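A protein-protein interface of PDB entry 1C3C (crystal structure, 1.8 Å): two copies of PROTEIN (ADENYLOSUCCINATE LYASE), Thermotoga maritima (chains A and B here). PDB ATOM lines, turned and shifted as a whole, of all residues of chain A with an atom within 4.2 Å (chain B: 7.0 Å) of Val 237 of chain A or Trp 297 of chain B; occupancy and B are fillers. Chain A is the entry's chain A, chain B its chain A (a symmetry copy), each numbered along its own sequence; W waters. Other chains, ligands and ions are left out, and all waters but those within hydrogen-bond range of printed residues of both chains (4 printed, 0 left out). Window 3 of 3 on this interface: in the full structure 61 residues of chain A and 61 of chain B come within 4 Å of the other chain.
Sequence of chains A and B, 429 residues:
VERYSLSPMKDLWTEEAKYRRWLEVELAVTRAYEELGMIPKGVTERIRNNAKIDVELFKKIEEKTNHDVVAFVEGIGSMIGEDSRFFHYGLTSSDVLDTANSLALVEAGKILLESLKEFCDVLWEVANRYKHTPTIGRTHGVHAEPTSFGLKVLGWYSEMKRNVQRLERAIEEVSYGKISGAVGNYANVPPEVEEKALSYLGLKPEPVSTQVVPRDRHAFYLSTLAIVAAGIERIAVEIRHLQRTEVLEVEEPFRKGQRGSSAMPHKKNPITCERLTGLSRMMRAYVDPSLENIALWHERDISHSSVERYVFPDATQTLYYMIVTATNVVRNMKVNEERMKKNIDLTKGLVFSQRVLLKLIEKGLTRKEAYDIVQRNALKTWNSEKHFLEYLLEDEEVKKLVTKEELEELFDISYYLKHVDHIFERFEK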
ATOM      1  N   GLU A 233     -19.041  23.945   7.359  1.00  0.00           N
ATOM      2  CA  GLU A 233     -18.224  22.731   7.496  1.00  0.00           C
ATOM      3  C   GLU A 233     -18.793  21.572   6.682  1.00  0.00           C
ATOM      4  O   GLU A 233     -18.024  20.790   6.093  1.00  0.00           O
ATOM      5  CB  GLU A 233     -18.167  22.402   9.009  1.00  0.00           C
ATOM      6  CG  GLU A 233     -17.328  21.179   9.389  1.00  0.00           C
ATOM      7  CD  GLU A 233     -17.579  20.821  10.857  1.00  0.00           C
ATOM      8  OE1 GLU A 233     -18.307  21.554  11.614  1.00  0.00           O
ATOM      9  OE2 GLU A 233     -17.039  19.775  11.268  1.00  0.00           O
ATOM     10  N   ARG A 234     -20.135  21.459   6.697  1.00  0.00           N
ATOM     11  CA  ARG A 234     -20.770  20.368   5.920  1.00  0.00           C
ATOM     12  C   ARG A 234     -20.404  20.480   4.440  1.00  0.00           C
ATOM     13  O   ARG A 234     -20.127  19.477   3.763  1.00  0.00           O
ATOM     14  CB  ARG A 234     -22.307  20.442   6.102  1.00  0.00           C
ATOM     15  CG  ARG A 234     -22.967  19.229   5.363  1.00  0.00           C
ATOM     16  CD  ARG A 234     -24.409  19.076   5.862  1.00  0.00           C
ATOM     17  NE  ARG A 234     -25.333  20.070   5.276  1.00  0.00           N
ATOM     18  CZ  ARG A 234     -26.024  19.824   4.159  1.00  0.00           C
ATOM     19  NH1 ARG A 234     -25.834  18.665   3.518  1.00  0.00           N
ATOM     20  NH2 ARG A 234     -26.894  20.721   3.683  1.00  0.00           N
ATOM     21  N   ILE A 235     -20.450  21.684   3.892  1.00  0.00           N
ATOM     22  CA  ILE A 235     -20.091  21.938   2.504  1.00  0.00           C
ATOM     23  C   ILE A 235     -18.599  21.650   2.259  1.00  0.00           C
ATOM     24  O   ILE A 235     -18.213  20.987   1.277  1.00  0.00           O
ATOM     25  CB  ILE A 235     -20.399  23.401   2.098  1.00  0.00           C
ATOM     26  CG1 ILE A 235     -21.905  23.690   2.267  1.00  0.00           C
ATOM     27  CG2 ILE A 235     -19.905  23.641   0.662  1.00  0.00           C
ATOM     28  CD1 ILE A 235     -22.287  25.182   2.127  1.00  0.00           C
ATOM     29  N   ALA A 236     -17.740  22.159   3.146  1.00  0.00           N
ATOM     30  CA  ALA A 236     -16.306  21.916   3.023  1.00  0.00           C
ATOM     31  C   ALA A 236     -15.995  20.419   3.072  1.00  0.00           C
ATOM     32  O   ALA A 236     -15.148  20.025   2.292  1.00  0.00           O
ATOM     33  CB  ALA A 236     -15.532  22.626   4.144  1.00  0.00           C
ATOM     34  N   VAL A 237     -16.645  19.614   3.939  1.00  0.00           N
ATOM     35  CA  VAL A 237     -16.341  18.190   4.015  1.00  0.00           C
ATOM     36  C   VAL A 237     -16.777  17.502   2.716  1.00  0.00           C
ATOM     37  O   VAL A 237     -16.074  16.657   2.160  1.00  0.00           O
ATOM     38  CB  VAL A 237     -17.028  17.572   5.247  1.00  0.00           C
ATOM     39  CG1 VAL A 237     -16.997  16.038   5.215  1.00  0.00           C
ATOM     40  CG2 VAL A 237     -16.206  18.030   6.487  1.00  0.00           C
ATOM     41  N   GLU A 238     -17.907  17.970   2.163  1.00  0.00           N
ATOM     42  CA  GLU A 238     -18.355  17.405   0.876  1.00  0.00           C
ATOM     43  C   GLU A 238     -17.295  17.684  -0.188  1.00  0.00           C
ATOM     44  O   GLU A 238     -16.960  16.761  -0.939  1.00  0.00           O
ATOM     45  CB  GLU A 238     -19.686  18.042   0.441  1.00  0.00           C
ATOM     46  CG  GLU A 238     -20.159  17.456  -0.920  1.00  0.00           C
ATOM     47  CD  GLU A 238     -20.825  16.103  -0.767  1.00  0.00           C
ATOM     48  OE1 GLU A 238     -20.845  15.288  -1.731  1.00  0.00           O
ATOM     49  OE2 GLU A 238     -21.316  15.873   0.354  1.00  0.00           O
ATOM     50  N   ILE A 239     -16.800  18.908  -0.293  1.00  0.00           N
ATOM     51  CA  ILE A 239     -15.807  19.220  -1.359  1.00  0.00           C
ATOM     52  C   ILE A 239     -14.532  18.436  -1.135  1.00  0.00           C
ATOM     53  O   ILE A 239     -13.912  17.907  -2.082  1.00  0.00           O
ATOM     54  CB  ILE A 239     -15.565  20.741  -1.388  1.00  0.00           C
ATOM     55  CG1 ILE A 239     -16.899  21.349  -1.903  1.00  0.00           C
ATOM     56  CG2 ILE A 239     -14.402  21.142  -2.313  1.00  0.00           C
ATOM     57  CD1 ILE A 239     -16.914  22.870  -1.839  1.00  0.00           C
ATOM     58  N   ARG A 240     -14.109  18.258   0.129  1.00  0.00           N
ATOM     59  CA  ARG A 240     -12.936  17.415   0.396  1.00  0.00           C
ATOM     60  C   ARG A 240     -13.113  15.994  -0.115  1.00  0.00           C
ATOM     61  O   ARG A 240     -12.183  15.414  -0.682  1.00  0.00           O
ATOM     62  CB  ARG A 240     -12.739  17.366   1.934  1.00  0.00           C
ATOM     63  CG  ARG A 240     -12.117  18.701   2.399  1.00  0.00           C
ATOM     64  CD  ARG A 240     -12.184  18.794   3.929  1.00  0.00           C
ATOM     65  NE  ARG A 240     -11.336  17.770   4.546  1.00  0.00           N
ATOM     66  CZ  ARG A 240     -11.343  17.467   5.830  1.00  0.00           C
ATOM     67  NH1 ARG A 240     -10.491  16.494   6.201  1.00  0.00           N
ATOM     68  NH2 ARG A 240     -12.121  18.113   6.732  1.00  0.00           N
ATOM     69  N   HIS A 241     -14.269  15.389   0.148  1.00  0.00           N
ATOM     70  CA  HIS A 241     -14.501  14.042  -0.368  1.00  0.00           C
ATOM     71  C   HIS A 241     -14.496  14.029  -1.908  1.00  0.00           C
ATOM     72  O   HIS A 241     -13.962  13.098  -2.515  1.00  0.00           O
ATOM     73  CB  HIS A 241     -15.892  13.552   0.050  1.00  0.00           C
ATOM     74  CG  HIS A 241     -16.041  13.180   1.493  1.00  0.00           C
ATOM     75  ND1 HIS A 241     -15.235  12.185   2.053  1.00  0.00           N
ATOM     76  CD2 HIS A 241     -16.881  13.576   2.461  1.00  0.00           C
ATOM     77  CE1 HIS A 241     -15.569  11.995   3.307  1.00  0.00           C
ATOM     78  NE2 HIS A 241     -16.580  12.835   3.584  1.00  0.00           N
ATOM     79  N   THR A 277     -12.941  23.543   7.730  1.00  0.00           N
ATOM     80  CA  THR A 277     -13.371  22.544   8.729  1.00  0.00           C
ATOM     81  C   THR A 277     -12.786  22.868  10.103  1.00  0.00           C
ATOM     82  O   THR A 277     -13.478  22.850  11.123  1.00  0.00           O
ATOM     83  CB  THR A 277     -12.927  21.149   8.265  1.00  0.00           C
ATOM     84  OG1 THR A 277     -13.433  20.918   6.931  1.00  0.00           O
ATOM     85  CG2 THR A 277     -13.447  20.047   9.194  1.00  0.00           C
ATOM     86  N   ILE B 294     -23.881  17.868  12.416  1.00  0.00           N
ATOM     87  CA  ILE B 294     -24.344  18.540  11.200  1.00  0.00           C
ATOM     88  C   ILE B 294     -23.580  18.101   9.964  1.00  0.00           C
ATOM     89  O   ILE B 294     -24.180  17.904   8.895  1.00  0.00           O
ATOM     90  CB  ILE B 294     -24.247  20.085  11.382  1.00  0.00           C
ATOM     91  CG1 ILE B 294     -25.307  20.451  12.469  1.00  0.00           C
ATOM     92  CG2 ILE B 294     -24.557  20.865  10.115  1.00  0.00           C
ATOM     93  CD1 ILE B 294     -25.129  21.873  13.001  1.00  0.00           C
ATOM     94  N   ALA B 295     -22.258  17.917  10.063  1.00  0.00           N
ATOM     95  CA  ALA B 295     -21.424  17.657   8.908  1.00  0.00           C
ATOM     96  C   ALA B 295     -21.375  16.160   8.587  1.00  0.00           C
ATOM     97  O   ALA B 295     -20.337  15.487   8.586  1.00  0.00           O
ATOM     98  CB  ALA B 295     -20.034  18.269   9.139  1.00  0.00           C
ATOM     99  N   LEU B 296     -22.547  15.613   8.226  1.00  0.00           N
ATOM    100  CA  LEU B 296     -22.669  14.245   7.750  1.00  0.00           C
ATOM    101  C   LEU B 296     -22.076  14.117   6.343  1.00  0.00           C
ATOM    102  O   LEU B 296     -22.140  15.077   5.547  1.00  0.00           O
ATOM    103  CB  LEU B 296     -24.173  13.916   7.693  1.00  0.00           C
ATOM    104  CG  LEU B 296     -24.889  13.912   9.047  1.00  0.00           C
ATOM    105  CD1 LEU B 296     -26.344  13.473   8.813  1.00  0.00           C
ATOM    106  CD2 LEU B 296     -24.241  12.954  10.043  1.00  0.00           C
ATOM    107  N   TRP B 297     -21.562  12.947   6.035  1.00  0.00           N
ATOM    108  CA  TRP B 297     -20.955  12.681   4.735  1.00  0.00           C
ATOM    109  C   TRP B 297     -22.026  12.479   3.667  1.00  0.00           C
ATOM    110  O   TRP B 297     -22.898  11.606   3.762  1.00  0.00           O
ATOM    111  CB  TRP B 297     -20.049  11.449   4.810  1.00  0.00           C
ATOM    112  CG  TRP B 297     -18.808  11.634   5.663  1.00  0.00           C
ATOM    113  CD1 TRP B 297     -18.480  12.636   6.515  1.00  0.00           C
ATOM    114  CD2 TRP B 297     -17.712  10.707   5.686  1.00  0.00           C
ATOM    115  NE1 TRP B 297     -17.227  12.392   7.105  1.00  0.00           N
ATOM    116  CE2 TRP B 297     -16.758  11.215   6.600  1.00  0.00           C
ATOM    117  CE3 TRP B 297     -17.454   9.481   5.054  1.00  0.00           C
ATOM    118  CZ2 TRP B 297     -15.541  10.568   6.879  1.00  0.00           C
ATOM    119  CZ3 TRP B 297     -16.242   8.833   5.308  1.00  0.00           C
ATOM    120  CH2 TRP B 297     -15.336   9.370   6.226  1.00  0.00           C
ATOM    121  N   HIS B 298     -21.900  13.279   2.606  1.00  0.00           N
ATOM    122  CA  HIS B 298     -22.710  13.165   1.403  1.00  0.00           C
ATOM    123  C   HIS B 298     -24.213  13.126   1.757  1.00  0.00           C
ATOM    124  O   HIS B 298     -24.677  13.990   2.500  1.00  0.00           O
ATOM    125  CB  HIS B 298     -22.301  11.945   0.595  1.00  0.00           C
ATOM    126  CG  HIS B 298     -20.865  11.920   0.128  1.00  0.00           C
ATOM    127  ND1 HIS B 298     -20.297  12.867  -0.680  1.00  0.00           N
ATOM    128  CD2 HIS B 298     -19.902  11.009   0.389  1.00  0.00           C
ATOM    129  CE1 HIS B 298     -19.028  12.516  -0.959  1.00  0.00           C
ATOM    130  NE2 HIS B 298     -18.758  11.415  -0.302  1.00  0.00           N
ATOM    131  N   GLU B 299     -24.947  12.137   1.246  1.00  0.00           N
ATOM    132  CA  GLU B 299     -26.394  12.037   1.498  1.00  0.00           C
ATOM    133  C   GLU B 299     -26.727  11.370   2.815  1.00  0.00           C
ATOM    134  O   GLU B 299     -27.929  11.233   3.120  1.00  0.00           O
ATOM    135  CB  GLU B 299     -27.064  11.335   0.291  1.00  0.00           C
ATOM    136  CG  GLU B 299     -27.159  12.262  -0.943  1.00  0.00           C
ATOM    137  CD  GLU B 299     -25.847  12.717  -1.526  1.00  0.00           C
ATOM    138  OE1 GLU B 299     -24.924  11.907  -1.858  1.00  0.00           O
ATOM    139  OE2 GLU B 299     -25.523  13.955  -1.675  1.00  0.00           O
ATOM    140  N   ARG B 300     -25.736  10.993   3.620  1.00  0.00           N
ATOM    141  CA  ARG B 300     -25.806  10.783   5.054  1.00  0.00           C
ATOM    142  C   ARG B 300     -24.764   9.754   5.506  1.00  0.00           C
ATOM    143  O   ARG B 300     -24.356   8.873   4.721  1.00  0.00           O
ATOM    144  CB  ARG B 300     -27.143  10.340   5.665  1.00  0.00           C
ATOM    145  CG  ARG B 300     -27.588   8.910   5.322  1.00  0.00           C
ATOM    146  CD  ARG B 300     -27.148   7.858   6.323  1.00  0.00           C
ATOM    147  NE  ARG B 300     -27.763   8.139   7.656  1.00  0.00           N
ATOM    148  CZ  ARG B 300     -28.997   7.840   7.999  1.00  0.00           C
ATOM    149  NH1 ARG B 300     -29.879   7.223   7.198  1.00  0.00           N
ATOM    150  NH2 ARG B 300     -29.453   8.206   9.216  1.00  0.00           N
ATOM    151  N   ASP B 301     -24.322   9.874   6.775  1.00  0.00           N
ATOM    152  CA  ASP B 301     -23.745   8.694   7.427  1.00  0.00           C
ATOM    153  C   ASP B 301     -24.563   8.511   8.717  1.00  0.00           C
ATOM    154  O   ASP B 301     -25.388   9.391   8.977  1.00  0.00           O
ATOM    155  CB  ASP B 301     -22.246   8.928   7.668  1.00  0.00           C
ATOM    156  CG  ASP B 301     -21.930  10.036   8.665  1.00  0.00           C
ATOM    157  OD1 ASP B 301     -22.246   9.842   9.850  1.00  0.00           O
ATOM    158  OD2 ASP B 301     -21.349  11.073   8.254  1.00  0.00           O
ATOM    159  N   SER B 303     -23.514   8.317  11.921  1.00  0.00           N
ATOM    160  CA  SER B 303     -22.819   8.679  13.168  1.00  0.00           C
ATOM    161  C   SER B 303     -23.736   9.434  14.130  1.00  0.00           C
ATOM    162  O   SER B 303     -23.626   9.230  15.341  1.00  0.00           O
ATOM    163  CB  SER B 303     -21.562   9.520  12.891  1.00  0.00           C
ATOM    164  OG  SER B 303     -21.951  10.727  12.240  1.00  0.00           O
HETATM  165  O   HOH W   1     -20.632  19.541  12.138  1.00  0.00           O
HETATM  166  O   HOH W   2     -20.291  16.885   4.518  1.00  0.00           O
HETATM  167  O   HOH W   3     -23.938  16.357   3.758  1.00  0.00           O
HETATM  168  O   HOH W   4     -19.863  15.149   2.528  1.00  0.00           O
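Among the printed residues, pairs that only touch across the chains: Glu 233 of chain A with Ala 295 of chain B, Arg 234 of chain A with Ile 294 of chain B, Arg 234 of chain A with Ala 295 of chain B, Val 237 of chain A with Trp 297 of chain B, His 241 of chain A with Trp 297 of chain B and His 241 of chain A with His 298 of chain B.
Water W2 bridges O of Arg 234 of chain A and O of Leu 296 of chain B. Water W4 bridges OE2 of Glu 238 of chain A (2.7 Å) and N of His 298 of chain B (2.8 Å). Water W3 lies within hydrogen-bond range of O of His 298 of chain B (2.8 Å), O of Leu 296 of chain B (2.8 Å) and NH1 of Arg 234 of chain A (3.0 Å). Water W1 lies within hydrogen-bond range of the backbone NH of Ala 295 of chain B (3.1 Å) and the side-chain carboxylate of Glu 233 of chain A (3.1 Å).
No position is printed for both chains.
A ring nitrogen (ND1) of His 298 of chain B is in hydrogen-bond range of the side-chain carboxylate of Glu 238 of chain A (2.7 Å).
OD2 of Asp 301 of chain B lies within hydrogen-bond range of N of Trp 297 of chain B.
Val 237 of chain A touches just one residue of chain B: Trp 297. Of the printed residues of chain A, Ala 295 of chain B touches Glu 233 and Arg 234. Of the printed residues of chain A, Ile 294 of chain B touches Arg 234 (3.3 Å). Of the printed residues of chain B, Glu 233 of chain A touches Ala 295 (3.9 Å). Printed residues of chain B within 4 Å of Arg 234 of chain A: Ile 294 and Ala 295. Ser 303 of chain B touches none of the printed residues of chain A. Thr 277 of chain A touches none of the printed residues of chain B. The nearest residue of chain B that does not touch Val 237 of chain A is Ala 295 of chain B (4.7 Å).
Hydrophobic or aromatic side chains of chain B that line the printed part of chain A: Ala 295, Trp 297 and His 298. Among the printed residues, 7 pairs touch across the chains.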
